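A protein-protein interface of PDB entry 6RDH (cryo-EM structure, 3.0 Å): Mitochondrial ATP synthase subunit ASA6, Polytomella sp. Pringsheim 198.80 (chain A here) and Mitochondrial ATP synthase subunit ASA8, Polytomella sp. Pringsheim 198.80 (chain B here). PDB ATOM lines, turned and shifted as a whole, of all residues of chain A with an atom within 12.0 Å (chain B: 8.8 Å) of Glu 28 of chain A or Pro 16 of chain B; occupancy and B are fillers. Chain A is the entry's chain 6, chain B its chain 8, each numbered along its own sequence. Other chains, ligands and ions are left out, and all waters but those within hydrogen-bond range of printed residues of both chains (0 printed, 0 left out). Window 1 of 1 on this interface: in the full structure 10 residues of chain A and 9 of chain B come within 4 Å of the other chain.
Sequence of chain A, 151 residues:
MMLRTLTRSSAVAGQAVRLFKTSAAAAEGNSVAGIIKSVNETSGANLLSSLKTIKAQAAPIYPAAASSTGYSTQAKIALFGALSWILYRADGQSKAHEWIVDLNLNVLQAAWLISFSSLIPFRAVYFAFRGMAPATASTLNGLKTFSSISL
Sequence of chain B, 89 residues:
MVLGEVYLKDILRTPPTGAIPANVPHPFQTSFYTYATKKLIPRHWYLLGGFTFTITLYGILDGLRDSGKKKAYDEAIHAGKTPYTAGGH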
ATOM      1  N   GLU A  28      -8.154  32.600   6.035  1.00  0.00           N
ATOM      2  CA  GLU A  28      -7.195  31.512   6.158  1.00  0.00           C
ATOM      3  C   GLU A  28      -6.664  31.095   4.791  1.00  0.00           C
ATOM      4  O   GLU A  28      -7.328  30.372   4.052  1.00  0.00           O
ATOM      5  CB  GLU A  28      -7.838  30.321   6.859  1.00  0.00           C
ATOM      6  CG  GLU A  28      -6.891  29.180   7.143  1.00  0.00           C
ATOM      7  CD  GLU A  28      -7.625  27.880   7.382  1.00  0.00           C
ATOM      8  OE1 GLU A  28      -8.724  27.712   6.817  1.00  0.00           O
ATOM      9  OE2 GLU A  28      -7.107  27.029   8.130  1.00  0.00           O
ATOM     10  N   GLY A  29      -5.466  31.565   4.457  1.00  0.00           N
ATOM     11  CA  GLY A  29      -4.853  31.226   3.192  1.00  0.00           C
ATOM     12  C   GLY A  29      -4.361  29.799   3.182  1.00  0.00           C
ATOM     13  O   GLY A  29      -4.324  29.115   4.203  1.00  0.00           O
ATOM     14  N   ASN A  30      -3.977  29.334   2.001  1.00  0.00           N
ATOM     15  CA  ASN A  30      -3.635  27.929   1.879  1.00  0.00           C
ATOM     16  C   ASN A  30      -2.229  27.673   2.393  1.00  0.00           C
ATOM     17  O   ASN A  30      -1.340  28.515   2.285  1.00  0.00           O
ATOM     18  CB  ASN A  30      -3.803  27.443   0.438  1.00  0.00           C
ATOM     19  CG  ASN A  30      -2.711  27.888  -0.463  1.00  0.00           C
ATOM     20  OD1 ASN A  30      -2.277  29.023  -0.402  1.00  0.00           O
ATOM     21  ND2 ASN A  30      -2.266  26.997  -1.329  1.00  0.00           N
ATOM     22  N   SER A  31      -2.047  26.499   2.984  1.00  0.00           N
ATOM     23  CA  SER A  31      -0.872  26.219   3.789  1.00  0.00           C
ATOM     24  C   SER A  31       0.379  25.993   2.969  1.00  0.00           C
ATOM     25  O   SER A  31       1.477  26.057   3.521  1.00  0.00           O
ATOM     26  CB  SER A  31      -1.130  25.000   4.663  1.00  0.00           C
ATOM     27  OG  SER A  31      -1.315  23.847   3.870  1.00  0.00           O
ATOM     28  N   VAL A  32       0.253  25.737   1.673  1.00  0.00           N
ATOM     29  CA  VAL A  32       1.439  25.595   0.842  1.00  0.00           C
ATOM     30  C   VAL A  32       2.067  26.954   0.572  1.00  0.00           C
ATOM     31  O   VAL A  32       3.292  27.092   0.589  1.00  0.00           O
ATOM     32  CB  VAL A  32       1.082  24.839  -0.445  1.00  0.00           C
ATOM     33  CG1 VAL A  32       2.212  24.843  -1.393  1.00  0.00           C
ATOM     34  CG2 VAL A  32       0.778  23.428  -0.101  1.00  0.00           C
ATOM     35  N   ALA A  33       1.255  27.988   0.355  1.00  0.00           N
ATOM     36  CA  ALA A  33       1.814  29.330   0.262  1.00  0.00           C
ATOM     37  C   ALA A  33       2.374  29.797   1.594  1.00  0.00           C
ATOM     38  O   ALA A  33       3.334  30.571   1.621  1.00  0.00           O
ATOM     39  CB  ALA A  33       0.773  30.319  -0.232  1.00  0.00           C
ATOM     40  N   GLY A  34       1.809  29.321   2.701  1.00  0.00           N
ATOM     41  CA  GLY A  34       2.424  29.564   3.992  1.00  0.00           C
ATOM     42  C   GLY A  34       3.767  28.882   4.139  1.00  0.00           C
ATOM     43  O   GLY A  34       4.695  29.458   4.704  1.00  0.00           O
ATOM     44  N   ILE A  35       3.898  27.659   3.617  1.00  0.00           N
ATOM     45  CA  ILE A  35       5.187  26.967   3.617  1.00  0.00           C
ATOM     46  C   ILE A  35       6.189  27.694   2.737  1.00  0.00           C
ATOM     47  O   ILE A  35       7.345  27.878   3.119  1.00  0.00           O
ATOM     48  CB  ILE A  35       5.013  25.498   3.184  1.00  0.00           C
ATOM     49  CG1 ILE A  35       4.377  24.684   4.296  1.00  0.00           C
ATOM     50  CG2 ILE A  35       6.318  24.860   2.799  1.00  0.00           C
ATOM     51  CD1 ILE A  35       4.038  23.287   3.889  1.00  0.00           C
ATOM     52  N   LYS A  37       6.229  30.920   1.813  1.00  0.00           N
ATOM     53  CA  LYS A  37       6.628  32.168   2.450  1.00  0.00           C
ATOM     54  C   LYS A  37       7.515  31.919   3.661  1.00  0.00           C
ATOM     55  O   LYS A  37       8.563  32.544   3.798  1.00  0.00           O
ATOM     56  CB  LYS A  37       5.398  32.971   2.844  1.00  0.00           C
ATOM     57  CG  LYS A  37       5.686  34.423   3.105  1.00  0.00           C
ATOM     58  CD  LYS A  37       4.531  35.102   3.813  1.00  0.00           C
ATOM     59  CE  LYS A  37       4.391  34.610   5.243  1.00  0.00           C
ATOM     60  NZ  LYS A  37       5.561  34.958   6.089  1.00  0.00           N
ATOM     61  N   ILE A  54       7.798  24.825  10.520  1.00  0.00           N
ATOM     62  CA  ILE A  54       6.978  25.037   9.333  1.00  0.00           C
ATOM     63  C   ILE A  54       6.191  23.782   8.991  1.00  0.00           C
ATOM     64  O   ILE A  54       5.106  23.864   8.409  1.00  0.00           O
ATOM     65  CB  ILE A  54       7.849  25.498   8.157  1.00  0.00           C
ATOM     66  CG1 ILE A  54       8.837  26.554   8.621  1.00  0.00           C
ATOM     67  CG2 ILE A  54       7.006  26.126   7.092  1.00  0.00           C
ATOM     68  CD1 ILE A  54       9.806  26.970   7.568  1.00  0.00           C
ATOM     69  N   LYS A  55       6.708  22.611   9.347  1.00  0.00           N
ATOM     70  CA  LYS A  55       5.947  21.382   9.172  1.00  0.00           C
ATOM     71  C   LYS A  55       4.729  21.359  10.082  1.00  0.00           C
ATOM     72  O   LYS A  55       3.651  20.924   9.670  1.00  0.00           O
ATOM     73  CB  LYS A  55       6.843  20.182   9.447  1.00  0.00           C
ATOM     74  CG  LYS A  55       6.172  18.840   9.338  1.00  0.00           C
ATOM     75  CD  LYS A  55       6.109  18.380   7.908  1.00  0.00           C
ATOM     76  CE  LYS A  55       5.877  16.885   7.841  1.00  0.00           C
ATOM     77  NZ  LYS A  55       6.101  16.339   6.474  1.00  0.00           N
ATOM     78  N   ALA A  56       4.871  21.846  11.313  1.00  0.00           N
ATOM     79  CA  ALA A  56       3.760  21.850  12.250  1.00  0.00           C
ATOM     80  C   ALA A  56       2.850  23.055  12.089  1.00  0.00           C
ATOM     81  O   ALA A  56       1.705  23.005  12.534  1.00  0.00           O
ATOM     82  CB  ALA A  56       4.284  21.797  13.681  1.00  0.00           C
ATOM     83  N   GLN A  57       3.327  24.140  11.481  1.00  0.00           N
ATOM     84  CA  GLN A  57       2.460  25.278  11.207  1.00  0.00           C
ATOM     85  C   GLN A  57       1.481  25.004  10.083  1.00  0.00           C
ATOM     86  O   GLN A  57       0.459  25.687   9.992  1.00  0.00           O
ATOM     87  CB  GLN A  57       3.277  26.506  10.828  1.00  0.00           C
ATOM     88  CG  GLN A  57       3.593  27.444  11.953  1.00  0.00           C
ATOM     89  CD  GLN A  57       4.210  28.727  11.444  1.00  0.00           C
ATOM     90  OE1 GLN A  57       4.184  29.002  10.245  1.00  0.00           O
ATOM     91  NE2 GLN A  57       4.775  29.517  12.347  1.00  0.00           N
ATOM     92  N   ALA A  58       1.780  24.051   9.210  1.00  0.00           N
ATOM     93  CA  ALA A  58       0.944  23.760   8.058  1.00  0.00           C
ATOM     94  C   ALA A  58       0.313  22.380   8.120  1.00  0.00           C
ATOM     95  O   ALA A  58      -0.320  21.959   7.151  1.00  0.00           O
ATOM     96  CB  ALA A  58       1.750  23.898   6.777  1.00  0.00           C
ATOM     97  N   ALA A  59       0.487  21.660   9.215  1.00  0.00           N
ATOM     98  CA  ALA A  59      -0.271  20.442   9.418  1.00  0.00           C
ATOM     99  C   ALA A  59      -1.722  20.802   9.716  1.00  0.00           C
ATOM    100  O   ALA A  59      -1.975  21.780  10.422  1.00  0.00           O
ATOM    101  CB  ALA A  59       0.319  19.634  10.566  1.00  0.00           C
ATOM    102  N   PRO A  60      -2.688  20.047   9.191  1.00  0.00           N
ATOM    103  CA  PRO A  60      -4.094  20.434   9.335  1.00  0.00           C
ATOM    104  C   PRO A  60      -4.586  20.285  10.762  1.00  0.00           C
ATOM    105  O   PRO A  60      -3.997  19.580  11.579  1.00  0.00           O
ATOM    106  CB  PRO A  60      -4.814  19.464   8.402  1.00  0.00           C
ATOM    107  CG  PRO A  60      -3.927  18.312   8.321  1.00  0.00           C
ATOM    108  CD  PRO A  60      -2.549  18.838   8.367  1.00  0.00           C
ATOM    109  N   ILE A  61      -5.674  20.981  11.071  1.00  0.00           N
ATOM    110  CA  ILE A  61      -6.177  20.954  12.434  1.00  0.00           C
ATOM    111  C   ILE A  61      -7.016  19.704  12.633  1.00  0.00           C
ATOM    112  O   ILE A  61      -7.981  19.449  11.909  1.00  0.00           O
ATOM    113  CB  ILE A  61      -6.955  22.238  12.784  1.00  0.00           C
ATOM    114  CG1 ILE A  61      -7.567  22.102  14.172  1.00  0.00           C
ATOM    115  CG2 ILE A  61      -8.014  22.609  11.752  1.00  0.00           C
ATOM    116  CD1 ILE A  61      -8.157  23.367  14.722  1.00  0.00           C
ATOM    117  N   TYR A  62      -6.602  18.883  13.581  1.00  0.00           N
ATOM    118  CA  TYR A  62      -7.403  17.767  14.060  1.00  0.00           C
ATOM    119  C   TYR A  62      -7.799  18.151  15.469  1.00  0.00           C
ATOM    120  O   TYR A  62      -6.955  18.102  16.380  1.00  0.00           O
ATOM    121  CB  TYR A  62      -6.613  16.470  14.052  1.00  0.00           C
ATOM    122  CG  TYR A  62      -6.027  16.118  12.719  1.00  0.00           C
ATOM    123  CD1 TYR A  62      -6.756  16.268  11.563  1.00  0.00           C
ATOM    124  CD2 TYR A  62      -4.746  15.618  12.621  1.00  0.00           C
ATOM    125  CE1 TYR A  62      -6.227  15.934  10.349  1.00  0.00           C
ATOM    126  CE2 TYR A  62      -4.209  15.285  11.412  1.00  0.00           C
ATOM    127  CZ  TYR A  62      -4.955  15.446  10.283  1.00  0.00           C
ATOM    128  OH  TYR A  62      -4.416  15.112   9.074  1.00  0.00           O
ATOM    129  N   PRO A  63      -9.040  18.580  15.690  1.00  0.00           N
ATOM    130  CA  PRO A  63      -9.412  19.120  16.996  1.00  0.00           C
ATOM    131  C   PRO A  63      -9.426  18.041  18.061  1.00  0.00           C
ATOM    132  O   PRO A  63      -9.841  16.907  17.815  1.00  0.00           O
ATOM    133  CB  PRO A  63     -10.813  19.686  16.749  1.00  0.00           C
ATOM    134  CG  PRO A  63     -10.899  19.850  15.287  1.00  0.00           C
ATOM    135  CD  PRO A  63     -10.135  18.720  14.728  1.00  0.00           C
ATOM    136  N   ALA A  64      -8.923  18.394  19.238  1.00  0.00           N
ATOM    137  CA  ALA A  64      -8.758  17.433  20.309  1.00  0.00           C
ATOM    138  C   ALA A  64     -10.098  17.120  20.961  1.00  0.00           C
ATOM    139  O   ALA A  64     -11.096  17.817  20.771  1.00  0.00           O
ATOM    140  CB  ALA A  64      -7.772  17.955  21.347  1.00  0.00           C
ATOM    141  N   GLU B   5      -1.445  32.509  -5.679  1.00  0.00           N
ATOM    142  CA  GLU B   5      -2.493  32.299  -4.673  1.00  0.00           C
ATOM    143  C   GLU B   5      -3.780  33.068  -4.949  1.00  0.00           C
ATOM    144  O   GLU B   5      -4.743  32.950  -4.191  1.00  0.00           O
ATOM    145  CB  GLU B   5      -1.974  32.635  -3.272  1.00  0.00           C
ATOM    146  CG  GLU B   5      -2.520  31.785  -2.157  1.00  0.00           C
ATOM    147  CD  GLU B   5      -2.116  32.303  -0.792  1.00  0.00           C
ATOM    148  OE1 GLU B   5      -1.123  33.051  -0.707  1.00  0.00           O
ATOM    149  OE2 GLU B   5      -2.794  31.968   0.199  1.00  0.00           O
ATOM    150  N   LEU B  12      -8.856  25.808  -5.641  1.00  0.00           N
ATOM    151  CA  LEU B  12      -8.091  24.774  -4.964  1.00  0.00           C
ATOM    152  C   LEU B  12      -7.740  25.281  -3.582  1.00  0.00           C
ATOM    153  O   LEU B  12      -7.119  26.336  -3.450  1.00  0.00           O
ATOM    154  CB  LEU B  12      -6.815  24.435  -5.729  1.00  0.00           C
ATOM    155  CG  LEU B  12      -6.947  23.575  -6.974  1.00  0.00           C
ATOM    156  CD1 LEU B  12      -5.652  23.592  -7.716  1.00  0.00           C
ATOM    157  CD2 LEU B  12      -7.303  22.180  -6.587  1.00  0.00           C
ATOM    158  N   ARG B  13      -8.132  24.542  -2.559  1.00  0.00           N
ATOM    159  CA  ARG B  13      -7.730  24.858  -1.204  1.00  0.00           C
ATOM    160  C   ARG B  13      -7.001  23.666  -0.611  1.00  0.00           C
ATOM    161  O   ARG B  13      -7.100  22.545  -1.105  1.00  0.00           O
ATOM    162  CB  ARG B  13      -8.929  25.236  -0.343  1.00  0.00           C
ATOM    163  CG  ARG B  13      -9.807  26.300  -0.950  1.00  0.00           C
ATOM    164  CD  ARG B  13     -10.673  26.937   0.091  1.00  0.00           C
ATOM    165  NE  ARG B  13     -11.511  27.992  -0.454  1.00  0.00           N
ATOM    166  CZ  ARG B  13     -12.768  27.826  -0.835  1.00  0.00           C
ATOM    167  NH1 ARG B  13     -13.452  28.847  -1.310  1.00  0.00           N
ATOM    168  NH2 ARG B  13     -13.337  26.643  -0.744  1.00  0.00           N
ATOM    169  N   THR B  14      -6.252  23.925   0.435  1.00  0.00           N
ATOM    170  CA  THR B  14      -5.511  22.927   1.180  1.00  0.00           C
ATOM    171  C   THR B  14      -6.323  22.497   2.390  1.00  0.00           C
ATOM    172  O   THR B  14      -7.351  23.109   2.693  1.00  0.00           O
ATOM    173  CB  THR B  14      -4.167  23.511   1.591  1.00  0.00           C
ATOM    174  OG1 THR B  14      -4.394  24.738   2.279  1.00  0.00           O
ATOM    175  CG2 THR B  14      -3.330  23.755   0.376  1.00  0.00           C
ATOM    176  N   PRO B  15      -5.948  21.404   3.067  1.00  0.00           N
ATOM    177  CA  PRO B  15      -6.631  21.027   4.303  1.00  0.00           C
ATOM    178  C   PRO B  15      -6.537  22.117   5.349  1.00  0.00           C
ATOM    179  O   PRO B  15      -5.487  22.757   5.491  1.00  0.00           O
ATOM    180  CB  PRO B  15      -5.877  19.771   4.749  1.00  0.00           C
ATOM    181  CG  PRO B  15      -4.721  19.669   3.853  1.00  0.00           C
ATOM    182  CD  PRO B  15      -5.164  20.258   2.594  1.00  0.00           C
ATOM    183  N   PRO B  16      -7.623  22.374   6.073  1.00  0.00           N
ATOM    184  CA  PRO B  16      -7.687  23.575   6.904  1.00  0.00           C
ATOM    185  C   PRO B  16      -6.840  23.446   8.152  1.00  0.00           C
ATOM    186  O   PRO B  16      -6.709  22.372   8.735  1.00  0.00           O
ATOM    187  CB  PRO B  16      -9.175  23.681   7.246  1.00  0.00           C
ATOM    188  CG  PRO B  16      -9.671  22.316   7.156  1.00  0.00           C
ATOM    189  CD  PRO B  16      -8.889  21.630   6.096  1.00  0.00           C
ATOM    190  N   THR B  17      -6.234  24.563   8.536  1.00  0.00           N
ATOM    191  CA  THR B  17      -5.421  24.644   9.737  1.00  0.00           C
ATOM    192  C   THR B  17      -6.061  25.480  10.827  1.00  0.00           C
ATOM    193  O   THR B  17      -5.787  25.251  12.005  1.00  0.00           O
ATOM    194  CB  THR B  17      -4.047  25.234   9.406  1.00  0.00           C
ATOM    195  OG1 THR B  17      -4.216  26.401   8.598  1.00  0.00           O
ATOM    196  CG2 THR B  17      -3.225  24.241   8.631  1.00  0.00           C
ATOM    197  N   GLY B  18      -6.909  26.433  10.461  1.00  0.00           N
ATOM    198  CA  GLY B  18      -7.553  27.285  11.434  1.00  0.00           C
ATOM    199  C   GLY B  18      -8.631  26.570  12.210  1.00  0.00           C
ATOM    200  O   GLY B  18      -8.506  26.377  13.421  1.00  0.00           O
ATOM    201  N   ALA B  19      -9.693  26.176  11.521  1.00  0.00           N
ATOM    202  CA  ALA B  19     -10.779  25.420  12.119  1.00  0.00           C
ATOM    203  C   ALA B  19     -11.530  24.722  11.002  1.00  0.00           C
ATOM    204  O   ALA B  19     -11.547  25.197   9.865  1.00  0.00           O
ATOM    205  CB  ALA B  19     -11.730  26.315  12.918  1.00  0.00           C
ATOM    206  N   ILE B  20     -12.142  23.596  11.337  1.00  0.00           N
ATOM    207  CA  ILE B  20     -12.929  22.830  10.366  1.00  0.00           C
ATOM    208  C   ILE B  20     -14.175  23.625  10.001  1.00  0.00           C
ATOM    209  O   ILE B  20     -14.910  24.057  10.902  1.00  0.00           O
ATOM    210  CB  ILE B  20     -13.293  21.472  10.944  1.00  0.00           C
ATOM    211  CG1 ILE B  20     -12.031  20.693  11.244  1.00  0.00           C
ATOM    212  CG2 ILE B  20     -14.119  20.685   9.978  1.00  0.00           C
ATOM    213  CD1 ILE B  20     -12.290  19.379  11.833  1.00  0.00           C
ATOM    214  N   PRO B  21     -14.456  23.849   8.717  1.00  0.00           N
ATOM    215  CA  PRO B  21     -15.582  24.710   8.347  1.00  0.00           C
ATOM    216  C   PRO B  21     -16.935  24.052   8.542  1.00  0.00           C
ATOM    217  O   PRO B  21     -17.037  22.953   9.094  1.00  0.00           O
ATOM    218  CB  PRO B  21     -15.332  24.993   6.864  1.00  0.00           C
ATOM    219  CG  PRO B  21     -14.015  24.442   6.562  1.00  0.00           C
ATOM    220  CD  PRO B  21     -13.732  23.384   7.534  1.00  0.00           C
ATOM    221  N   ALA B  22     -17.985  24.724   8.102  1.00  0.00           N
ATOM    222  CA  ALA B  22     -19.295  24.111   8.047  1.00  0.00           C
ATOM    223  C   ALA B  22     -19.459  23.390   6.722  1.00  0.00           C
ATOM    224  O   ALA B  22     -18.837  23.747   5.722  1.00  0.00           O
ATOM    225  CB  ALA B  22     -20.389  25.159   8.213  1.00  0.00           C
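OE2 of Glu 5 of chain B lies close to OD1 of Asn 30 of chain A (3.0 Å). N of Ile 61 of chain A is in hydrogen-bond range of O of Pro 16 of chain B (2.9 Å). N of Ser 31 of chain A sits at hydrogen-bond distance from OG1 of Thr 14 of chain B (3.0 Å). The backbone NH (N) of Thr 17 of chain B is in hydrogen-bond range of the side-chain carboxylate (OE2) of Glu 28 of chain A (2.6 Å). The side-chain carboxylate (OE2) of Glu 28 of chain A lies within hydrogen-bond range of the backbone NH (N) of Gly 18 of chain B (2.4 Å).
Among the printed residues, merely in contact across the chains: Ala 59 of chain A with Thr 17 of chain B (3.3 Å), Ile 61 of chain A with Gly 18 of chain B (3.3 Å), Asn 30 of chain A with Thr 14 of chain B (3.3 Å), Pro 60 of chain A with Pro 16 of chain B (3.3 Å), Ile 61 of chain A with Thr 17 of chain B (3.3 Å), Ala 33 of chain A with Glu 5 of chain B (3.4 Å), Glu 28 of chain A with Pro 16 of chain B (3.6 Å), Pro 63 of chain A with Ile 20 of chain B (3.7 Å), Gly 29 of chain A with Glu 5 of chain B (3.7 Å), Pro 60 of chain A with Pro 15 of chain B (3.8 Å), Ile 61 of chain A with Ala 19 of chain B (3.9 Å), Pro 60 of chain A with Thr 17 of chain B (3.97 Å) and Ala 58 of chain A with Thr 17 of chain B (3.98 Å).
Of chain B, only Pro 16, Thr 17 and Gly 18 come within 4 Å of Glu 28 of chain A. Gly 29 of chain A touches just one residue of chain B: Glu 5. Of the printed residues of chain B, Asn 30 of chain A touches Glu 5 (3.0 Å) and Thr 14 (3.3 Å). Of the printed residues of chain B, Ser 31 of chain A touches Thr 14 (3.0 Å). Of the printed residues of chain B, Ala 58 of chain A touches Thr 17 (3.98 Å). Printed residues of chain B within 4 Å of Pro 60 of chain A: Pro 15 (3.8 Å), Pro 16 (3.3 Å) and Thr 17 (3.97 Å). Of the printed residues of chain B, Ile 61 of chain A touches Pro 16 (2.9 Å), Thr 17 (3.3 Å), Gly 18 (3.3 Å) and Ala 19 (3.9 Å). Of chain A, only Asn 30 (3.3 Å) and Ser 31 (3.0 Å) come within 4 Å of Thr 14 of chain B. Pro 16 of chain B touches just these residues of chain A: Glu 28, Pro 60 and Ile 61. Gly 18 of chain B touches just these residues of chain A: Glu 28 (2.4 Å) and Ile 61 (3.3 Å). Ala 19 of chain B touches just one residue of chain A: Ile 61 (3.9 Å). Of chain A, only Pro 63 comes within 4 Å of Ile 20 of chain B. No residue of chain A comes within 4 Å of Pro 21 of chain B. The nearest residue of chain A that does not touch Pro 16 of chain B is Ala 59 of chain A (5.1 Å). The nearest printed residue of chain A that does not touch Glu 5 of chain B is Gly 34 of chain A (5.8 Å).
Of the 20 printed residues of chain A, 10 touch a printed residue of chain B. Printed residues of chain A that touch a printed residue of chain B: Glu 28, Gly 29, Asn 30, Ser 31, Ala 33, Ala 58, Ala 59, Pro 60, Ile 61 and Pro 63. Hydrophobic or aromatic side chains of chain B within 4 Å of the printed part of chain A: Pro 15 and Ile 20. Among the printed residues, 18 pairs touch across the chains. Among the printed residues, no Asp or Glu carboxylate lies within 4 Å of a Lys or Arg side-chain nitrogen of the other chain.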
